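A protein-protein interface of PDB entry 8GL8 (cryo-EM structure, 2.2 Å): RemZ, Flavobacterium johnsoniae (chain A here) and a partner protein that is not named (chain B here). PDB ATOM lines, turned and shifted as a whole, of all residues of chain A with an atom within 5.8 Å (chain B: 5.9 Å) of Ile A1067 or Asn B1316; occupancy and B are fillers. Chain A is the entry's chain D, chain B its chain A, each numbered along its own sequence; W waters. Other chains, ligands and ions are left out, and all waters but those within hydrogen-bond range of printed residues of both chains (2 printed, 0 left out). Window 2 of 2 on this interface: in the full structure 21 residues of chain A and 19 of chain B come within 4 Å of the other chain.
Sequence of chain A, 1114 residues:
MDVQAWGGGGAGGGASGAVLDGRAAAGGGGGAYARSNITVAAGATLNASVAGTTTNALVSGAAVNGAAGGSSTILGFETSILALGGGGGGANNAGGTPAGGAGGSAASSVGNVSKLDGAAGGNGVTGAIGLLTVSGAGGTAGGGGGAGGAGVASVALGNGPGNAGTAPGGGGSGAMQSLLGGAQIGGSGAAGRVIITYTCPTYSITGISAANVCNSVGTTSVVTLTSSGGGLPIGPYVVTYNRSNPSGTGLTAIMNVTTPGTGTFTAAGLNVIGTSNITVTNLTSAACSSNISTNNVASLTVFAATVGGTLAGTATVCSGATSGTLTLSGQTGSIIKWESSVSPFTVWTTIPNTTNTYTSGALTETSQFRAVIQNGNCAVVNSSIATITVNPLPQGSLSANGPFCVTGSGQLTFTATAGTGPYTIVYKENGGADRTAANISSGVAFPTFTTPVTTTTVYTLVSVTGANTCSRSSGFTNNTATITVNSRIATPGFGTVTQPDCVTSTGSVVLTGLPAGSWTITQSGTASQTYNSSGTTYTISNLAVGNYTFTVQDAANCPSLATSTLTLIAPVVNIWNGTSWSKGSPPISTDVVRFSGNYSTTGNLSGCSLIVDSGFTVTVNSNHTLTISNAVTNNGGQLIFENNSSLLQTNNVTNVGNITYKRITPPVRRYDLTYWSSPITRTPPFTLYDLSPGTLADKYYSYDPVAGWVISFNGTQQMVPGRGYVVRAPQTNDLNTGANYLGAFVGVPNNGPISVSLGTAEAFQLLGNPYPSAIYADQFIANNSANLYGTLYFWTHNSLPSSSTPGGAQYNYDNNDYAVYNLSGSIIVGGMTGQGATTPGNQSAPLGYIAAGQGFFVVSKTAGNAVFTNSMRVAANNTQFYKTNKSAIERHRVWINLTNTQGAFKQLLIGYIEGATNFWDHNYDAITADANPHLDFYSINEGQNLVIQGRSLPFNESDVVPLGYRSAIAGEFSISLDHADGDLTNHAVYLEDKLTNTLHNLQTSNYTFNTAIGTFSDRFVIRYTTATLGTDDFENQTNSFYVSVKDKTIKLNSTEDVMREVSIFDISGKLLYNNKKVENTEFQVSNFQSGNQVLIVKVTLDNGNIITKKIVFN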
ATOM      1  N   PHE A1065       6.513 -11.235  -8.662  1.00  0.00           N
ATOM      2  CA  PHE A1065       5.592 -12.350  -8.519  1.00  0.00           C
ATOM      3  C   PHE A1065       6.352 -13.614  -8.143  1.00  0.00           C
ATOM      4  O   PHE A1065       7.540 -13.768  -8.448  1.00  0.00           O
ATOM      5  CB  PHE A1065       4.819 -12.621  -9.818  1.00  0.00           C
ATOM      6  CG  PHE A1065       3.929 -11.497 -10.255  1.00  0.00           C
ATOM      7  CD1 PHE A1065       4.433 -10.451 -11.007  1.00  0.00           C
ATOM      8  CD2 PHE A1065       2.584 -11.501  -9.935  1.00  0.00           C
ATOM      9  CE1 PHE A1065       3.612  -9.423 -11.418  1.00  0.00           C
ATOM     10  CE2 PHE A1065       1.758 -10.476 -10.345  1.00  0.00           C
ATOM     11  CZ  PHE A1065       2.273  -9.435 -11.087  1.00  0.00           C
ATOM     12  N   ASP A1066       5.637 -14.525  -7.497  1.00  0.00           N
ATOM     13  CA  ASP A1066       6.128 -15.861  -7.208  1.00  0.00           C
ATOM     14  C   ASP A1066       5.879 -16.792  -8.395  1.00  0.00           C
ATOM     15  O   ASP A1066       5.204 -16.443  -9.364  1.00  0.00           O
ATOM     16  CB  ASP A1066       5.455 -16.414  -5.953  1.00  0.00           C
ATOM     17  CG  ASP A1066       6.450 -16.958  -4.956  1.00  0.00           C
ATOM     18  OD1 ASP A1066       7.569 -17.320  -5.374  1.00  0.00           O
ATOM     19  OD2 ASP A1066       6.114 -17.025  -3.754  1.00  0.00           O
ATOM     20  N   ILE A1067       6.444 -17.997  -8.305  1.00  0.00           N
ATOM     21  CA  ILE A1067       6.174 -19.021  -9.309  1.00  0.00           C
ATOM     22  C   ILE A1067       4.709 -19.434  -9.269  1.00  0.00           C
ATOM     23  O   ILE A1067       4.126 -19.795 -10.298  1.00  0.00           O
ATOM     24  CB  ILE A1067       7.129 -20.214  -9.109  1.00  0.00           C
ATOM     25  CG1 ILE A1067       8.502 -19.890  -9.700  1.00  0.00           C
ATOM     26  CG2 ILE A1067       6.578 -21.486  -9.735  1.00  0.00           C
ATOM     27  CD1 ILE A1067       8.436 -19.309 -11.097  1.00  0.00           C
ATOM     28  N   SER A1068       4.077 -19.359  -8.097  1.00  0.00           N
ATOM     29  CA  SER A1068       2.649 -19.620  -7.990  1.00  0.00           C
ATOM     30  C   SER A1068       1.801 -18.566  -8.689  1.00  0.00           C
ATOM     31  O   SER A1068       0.595 -18.778  -8.854  1.00  0.00           O
ATOM     32  CB  SER A1068       2.244 -19.707  -6.518  1.00  0.00           C
ATOM     33  OG  SER A1068       2.065 -18.417  -5.961  1.00  0.00           O
ATOM     34  N   GLY A1069       2.394 -17.445  -9.099  1.00  0.00           N
ATOM     35  CA  GLY A1069       1.658 -16.348  -9.682  1.00  0.00           C
ATOM     36  C   GLY A1069       1.203 -15.298  -8.695  1.00  0.00           C
ATOM     37  O   GLY A1069       0.654 -14.272  -9.114  1.00  0.00           O
ATOM     38  N   LYS A1070       1.415 -15.518  -7.401  1.00  0.00           N
ATOM     39  CA  LYS A1070       1.002 -14.556  -6.390  1.00  0.00           C
ATOM     40  C   LYS A1070       1.882 -13.314  -6.450  1.00  0.00           C
ATOM     41  O   LYS A1070       3.111 -13.414  -6.519  1.00  0.00           O
ATOM     42  CB  LYS A1070       1.072 -15.191  -5.002  1.00  0.00           C
ATOM     43  CG  LYS A1070       1.071 -14.200  -3.852  1.00  0.00           C
ATOM     44  CD  LYS A1070       0.989 -14.915  -2.513  1.00  0.00           C
ATOM     45  CE  LYS A1070       2.215 -15.779  -2.272  1.00  0.00           C
ATOM     46  NZ  LYS A1070       2.499 -15.956  -0.823  1.00  0.00           N
ATOM     47  N   SER A1090       8.863 -19.279   2.207  1.00  0.00           N
ATOM     48  CA  SER A1090       8.458 -20.681   2.330  1.00  0.00           C
ATOM     49  C   SER A1090       9.094 -21.549   1.241  1.00  0.00           C
ATOM     50  O   SER A1090       8.414 -22.199   0.445  1.00  0.00           O
ATOM     51  CB  SER A1090       6.930 -20.812   2.318  1.00  0.00           C
ATOM     52  OG  SER A1090       6.327 -19.829   3.139  1.00  0.00           O
ATOM     53  N   ASN A1092      10.723 -20.768  -1.442  1.00  0.00           N
ATOM     54  CA  ASN A1092      10.666 -20.278  -2.811  1.00  0.00           C
ATOM     55  C   ASN A1092      11.902 -19.440  -3.110  1.00  0.00           C
ATOM     56  O   ASN A1092      12.264 -18.556  -2.327  1.00  0.00           O
ATOM     57  CB  ASN A1092       9.397 -19.458  -3.044  1.00  0.00           C
ATOM     58  CG  ASN A1092       8.143 -20.309  -3.023  1.00  0.00           C
ATOM     59  OD1 ASN A1092       8.122 -21.415  -3.562  1.00  0.00           O
ATOM     60  ND2 ASN A1092       7.091 -19.798  -2.396  1.00  0.00           N
ATOM     61  N   VAL A1094      12.815 -18.860  -6.933  1.00  0.00           N
ATOM     62  CA  VAL A1094      12.571 -18.254  -8.240  1.00  0.00           C
ATOM     63  C   VAL A1094      11.485 -17.191  -8.133  1.00  0.00           C
ATOM     64  O   VAL A1094      10.403 -17.436  -7.588  1.00  0.00           O
ATOM     65  CB  VAL A1094      12.199 -19.325  -9.276  1.00  0.00           C
ATOM     66  CG1 VAL A1094      12.000 -18.692 -10.643  1.00  0.00           C
ATOM     67  CG2 VAL A1094      13.274 -20.397  -9.336  1.00  0.00           C
ATOM     68  N   LEU A1095      11.775 -16.006  -8.667  1.00  0.00           N
ATOM     69  CA  LEU A1095      10.853 -14.882  -8.703  1.00  0.00           C
ATOM     70  C   LEU A1095      10.811 -14.306 -10.111  1.00  0.00           C
ATOM     71  O   LEU A1095      11.754 -14.453 -10.894  1.00  0.00           O
ATOM     72  CB  LEU A1095      11.262 -13.785  -7.715  1.00  0.00           C
ATOM     73  CG  LEU A1095      11.289 -14.169  -6.240  1.00  0.00           C
ATOM     74  CD1 LEU A1095      11.771 -13.001  -5.404  1.00  0.00           C
ATOM     75  CD2 LEU A1095       9.913 -14.614  -5.802  1.00  0.00           C
ATOM     76  N   ILE A1096       9.705 -13.635 -10.425  1.00  0.00           N
ATOM     77  CA  ILE A1096       9.515 -12.988 -11.718  1.00  0.00           C
ATOM     78  C   ILE A1096       9.373 -11.490 -11.490  1.00  0.00           C
ATOM     79  O   ILE A1096       8.511 -11.055 -10.719  1.00  0.00           O
ATOM     80  CB  ILE A1096       8.288 -13.550 -12.461  1.00  0.00           C
ATOM     81  CG1 ILE A1096       8.495 -15.032 -12.781  1.00  0.00           C
ATOM     82  CG2 ILE A1096       8.030 -12.766 -13.734  1.00  0.00           C
ATOM     83  CD1 ILE A1096       7.212 -15.821 -12.885  1.00  0.00           C
ATOM     84  N   LYS A1110      13.481 -13.353 -14.923  1.00  0.00           N
ATOM     85  CA  LYS A1110      13.416 -14.396 -13.911  1.00  0.00           C
ATOM     86  C   LYS A1110      14.691 -14.353 -13.083  1.00  0.00           C
ATOM     87  O   LYS A1110      15.795 -14.372 -13.635  1.00  0.00           O
ATOM     88  CB  LYS A1110      13.236 -15.773 -14.549  1.00  0.00           C
ATOM     89  CG  LYS A1110      11.796 -16.249 -14.583  1.00  0.00           C
ATOM     90  CD  LYS A1110      11.653 -17.537 -15.372  1.00  0.00           C
ATOM     91  CE  LYS A1110      11.991 -17.327 -16.838  1.00  0.00           C
ATOM     92  NZ  LYS A1110      11.218 -18.245 -17.717  1.00  0.00           N
ATOM     93  N   ILE B 949       4.882 -26.200   2.237  1.00  0.00           N
ATOM     94  CA  ILE B 949       6.031 -26.069   1.351  1.00  0.00           C
ATOM     95  C   ILE B 949       5.740 -26.856   0.083  1.00  0.00           C
ATOM     96  O   ILE B 949       5.307 -28.013   0.150  1.00  0.00           O
ATOM     97  CB  ILE B 949       7.327 -26.561   2.017  1.00  0.00           C
ATOM     98  CG1 ILE B 949       7.430 -26.040   3.452  1.00  0.00           C
ATOM     99  CG2 ILE B 949       8.537 -26.149   1.192  1.00  0.00           C
ATOM    100  CD1 ILE B 949       7.928 -24.618   3.557  1.00  0.00           C
ATOM    101  N   ALA B 950       5.962 -26.228  -1.067  1.00  0.00           N
ATOM    102  CA  ALA B 950       5.765 -26.909  -2.337  1.00  0.00           C
ATOM    103  C   ALA B 950       6.746 -28.065  -2.478  1.00  0.00           C
ATOM    104  O   ALA B 950       7.897 -27.984  -2.041  1.00  0.00           O
ATOM    105  CB  ALA B 950       5.933 -25.927  -3.495  1.00  0.00           C
ATOM    106  N   GLN B 953      10.818 -28.111  -3.128  1.00  0.00           N
ATOM    107  CA  GLN B 953      11.441 -26.903  -2.613  1.00  0.00           C
ATOM    108  C   GLN B 953      12.183 -27.223  -1.317  1.00  0.00           C
ATOM    109  O   GLN B 953      12.309 -28.382  -0.915  1.00  0.00           O
ATOM    110  CB  GLN B 953      10.393 -25.809  -2.422  1.00  0.00           C
ATOM    111  CG  GLN B 953       9.675 -25.412  -3.700  1.00  0.00           C
ATOM    112  CD  GLN B 953      10.631 -25.052  -4.820  1.00  0.00           C
ATOM    113  OE1 GLN B 953      10.531 -25.577  -5.928  1.00  0.00           O
ATOM    114  NE2 GLN B 953      11.562 -24.150  -4.537  1.00  0.00           N
ATOM    115  N   LEU B1314      -3.650 -21.420  -2.536  1.00  0.00           N
ATOM    116  CA  LEU B1314      -3.076 -21.189  -3.852  1.00  0.00           C
ATOM    117  C   LEU B1314      -2.423 -22.469  -4.357  1.00  0.00           C
ATOM    118  O   LEU B1314      -2.307 -23.461  -3.638  1.00  0.00           O
ATOM    119  CB  LEU B1314      -2.056 -20.045  -3.825  1.00  0.00           C
ATOM    120  CG  LEU B1314      -2.574 -18.670  -3.399  1.00  0.00           C
ATOM    121  CD1 LEU B1314      -1.418 -17.721  -3.140  1.00  0.00           C
ATOM    122  CD2 LEU B1314      -3.517 -18.100  -4.446  1.00  0.00           C
ATOM    123  N   TYR B1315      -2.008 -22.440  -5.618  1.00  0.00           N
ATOM    124  CA  TYR B1315      -1.276 -23.538  -6.234  1.00  0.00           C
ATOM    125  C   TYR B1315       0.134 -23.060  -6.545  1.00  0.00           C
ATOM    126  O   TYR B1315       0.319 -22.171  -7.383  1.00  0.00           O
ATOM    127  CB  TYR B1315      -1.978 -24.021  -7.504  1.00  0.00           C
ATOM    128  CG  TYR B1315      -2.892 -25.204  -7.287  1.00  0.00           C
ATOM    129  CD1 TYR B1315      -2.375 -26.466  -7.028  1.00  0.00           C
ATOM    130  CD2 TYR B1315      -4.271 -25.059  -7.338  1.00  0.00           C
ATOM    131  CE1 TYR B1315      -3.206 -27.549  -6.827  1.00  0.00           C
ATOM    132  CE2 TYR B1315      -5.110 -26.136  -7.138  1.00  0.00           C
ATOM    133  CZ  TYR B1315      -4.572 -27.380  -6.883  1.00  0.00           C
ATOM    134  OH  TYR B1315      -5.404 -28.457  -6.684  1.00  0.00           O
ATOM    135  N   ASN B1316       1.126 -23.643  -5.870  1.00  0.00           N
ATOM    136  CA  ASN B1316       2.509 -23.240  -6.102  1.00  0.00           C
ATOM    137  C   ASN B1316       3.072 -23.918  -7.346  1.00  0.00           C
ATOM    138  O   ASN B1316       3.417 -23.254  -8.329  1.00  0.00           O
ATOM    139  CB  ASN B1316       3.364 -23.562  -4.875  1.00  0.00           C
ATOM    140  CG  ASN B1316       4.521 -22.603  -4.707  1.00  0.00           C
ATOM    141  OD1 ASN B1316       5.102 -22.137  -5.685  1.00  0.00           O
ATOM    142  ND2 ASN B1316       4.863 -22.303  -3.461  1.00  0.00           N
ATOM    143  N   ASN B1317       3.175 -25.245  -7.314  1.00  0.00           N
ATOM    144  CA  ASN B1317       3.431 -26.032  -8.520  1.00  0.00           C
ATOM    145  C   ASN B1317       2.747 -27.384  -8.309  1.00  0.00           C
ATOM    146  O   ASN B1317       3.339 -28.318  -7.764  1.00  0.00           O
ATOM    147  CB  ASN B1317       4.920 -26.174  -8.805  1.00  0.00           C
ATOM    148  CG  ASN B1317       5.704 -26.671  -7.607  1.00  0.00           C
ATOM    149  OD1 ASN B1317       6.049 -25.898  -6.714  1.00  0.00           O
ATOM    150  ND2 ASN B1317       5.990 -27.967  -7.581  1.00  0.00           N
ATOM    151  N   ASN B1318       1.493 -27.469  -8.752  1.00  0.00           N
ATOM    152  CA  ASN B1318       0.643 -28.641  -8.560  1.00  0.00           C
ATOM    153  C   ASN B1318       0.514 -29.032  -7.089  1.00  0.00           C
ATOM    154  O   ASN B1318       0.182 -30.178  -6.774  1.00  0.00           O
ATOM    155  CB  ASN B1318       1.147 -29.827  -9.389  1.00  0.00           C
ATOM    156  CG  ASN B1318       1.802 -29.388 -10.685  1.00  0.00           C
ATOM    157  OD1 ASN B1318       1.164 -28.774 -11.538  1.00  0.00           O
ATOM    158  ND2 ASN B1318       3.087 -29.687 -10.830  1.00  0.00           N
ATOM    159  N   THR B1319       0.768 -28.093  -6.180  1.00  0.00           N
ATOM    160  CA  THR B1319       0.674 -28.324  -4.745  1.00  0.00           C
ATOM    161  C   THR B1319      -0.210 -27.252  -4.129  1.00  0.00           C
ATOM    162  O   THR B1319      -0.032 -26.062  -4.410  1.00  0.00           O
ATOM    163  CB  THR B1319       2.059 -28.309  -4.084  1.00  0.00           C
ATOM    164  OG1 THR B1319       2.918 -29.249  -4.740  1.00  0.00           O
ATOM    165  CG2 THR B1319       1.955 -28.670  -2.611  1.00  0.00           C
ATOM    166  N   VAL B1320      -1.156 -27.670  -3.294  1.00  0.00           N
ATOM    167  CA  VAL B1320      -2.036 -26.732  -2.606  1.00  0.00           C
ATOM    168  C   VAL B1320      -1.288 -26.148  -1.415  1.00  0.00           C
ATOM    169  O   VAL B1320      -0.782 -26.885  -0.564  1.00  0.00           O
ATOM    170  CB  VAL B1320      -3.337 -27.414  -2.161  1.00  0.00           C
ATOM    171  CG1 VAL B1320      -4.232 -26.421  -1.434  1.00  0.00           C
ATOM    172  CG2 VAL B1320      -4.058 -28.008  -3.357  1.00  0.00           C
ATOM    173  N   ILE B1321      -1.214 -24.822  -1.358  1.00  0.00           N
ATOM    174  CA  ILE B1321      -0.531 -24.105  -0.290  1.00  0.00           C
ATOM    175  C   ILE B1321      -1.565 -23.272   0.452  1.00  0.00           C
ATOM    176  O   ILE B1321      -2.246 -22.431  -0.153  1.00  0.00           O
ATOM    177  CB  ILE B1321       0.602 -23.217  -0.828  1.00  0.00           C
ATOM    178  CG1 ILE B1321       1.512 -24.016  -1.763  1.00  0.00           C
ATOM    179  CG2 ILE B1321       1.389 -22.603   0.320  1.00  0.00           C
ATOM    180  CD1 ILE B1321       2.532 -24.879  -1.049  1.00  0.00           C
HETATM  181  O   HOH W   1      11.236 -21.559  -6.694  1.00  0.00           O
HETATM  182  O   HOH W   2       7.246 -23.376  -1.362  1.00  0.00           O
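The side-chain amide nitrogen of Asn B1316 is in hydrogen-bond range of the side-chain amide oxygen of Asn A1092.
Water W2 lies within hydrogen-bond range of O of Ser A1090 (2.5 Å), OD1 of Asn A1092 (3.1 Å), N of Ala B950 (3.1 Å) and ND2 of Asn B1316 (3.4 Å).
Water W1 bridges the backbone NH of Val A1094 (3.1 Å) and the side-chain amide nitrogen of Gln B953 (3.4 Å).
Of the 11 printed residues of chain B, 4 touch a printed residue of chain A.
Hydrophobic or aromatic side chains of chain B within 4 Å of the printed part of chain A: Ile B949 and Leu B1314.
Of the 12 printed residues of chain A, 5 touch a printed residue of chain B.
Hydrophobic or aromatic side chains of chain A within 4 Å of the printed part of chain B: Ile A1067.
Among the printed residues, 6 pairs touch across the chains.
Among the printed residues, no Asp or Glu carboxylate lies within 4 Å of a Lys or Arg side-chain nitrogen of the other chain.
Printed residues of chain B within 4 Å of Ile A1067: Asn B1316 (3.9 Å).
Of the printed residues of chain A, Asn B1316 touches Ile A1067 (3.9 Å), Ser A1068 (3.6 Å) and Asn A1092 (3.4 Å).
Of the printed residues of chain B, Ser A1068 touches Tyr B1315 and Asn B1316.
Printed residues of chain B within 4 Å of Ser A1090: Ile B949.
Printed residues of chain A within 4 Å of Leu B1314: Lys A1070.
Printed residues of chain A within 4 Å of Tyr B1315: Ser A1068 (3.2 Å).
Ile A1096 touches none of the printed residues of chain B.
The nearest residue of chain B that does not touch Ile A1067 is Asn B1317 (5.1 Å).
The nearest printed residue of chain A that does not touch Asn B1316 is Ser A1090 (5.3 Å).
The nearest printed residue of chain A that does not touch Ile B949 is Asn A1092 (6.4 Å).
Among the printed residues, pairs that only touch across the chains: Ile A1067 with Asn B1316, Ser A1068 with Tyr B1315, Ser A1068 with Asn B1316, Lys A1070 with Leu B1314 and Ser A1090 with Ile B949.
The backbone carbonyl oxygen of Leu B1314 sits at hydrogen-bond distance from the backbone NH of Ile B1321, at 2.9 Å.
OG of Ser A1068 is in hydrogen-bond range of N of Lys A1070 (3.3 Å).
The side-chain carboxylate of Asp A1066 lies within hydrogen-bond range of the side-chain amide nitrogen of Asn A1092, 3.2 Å away.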
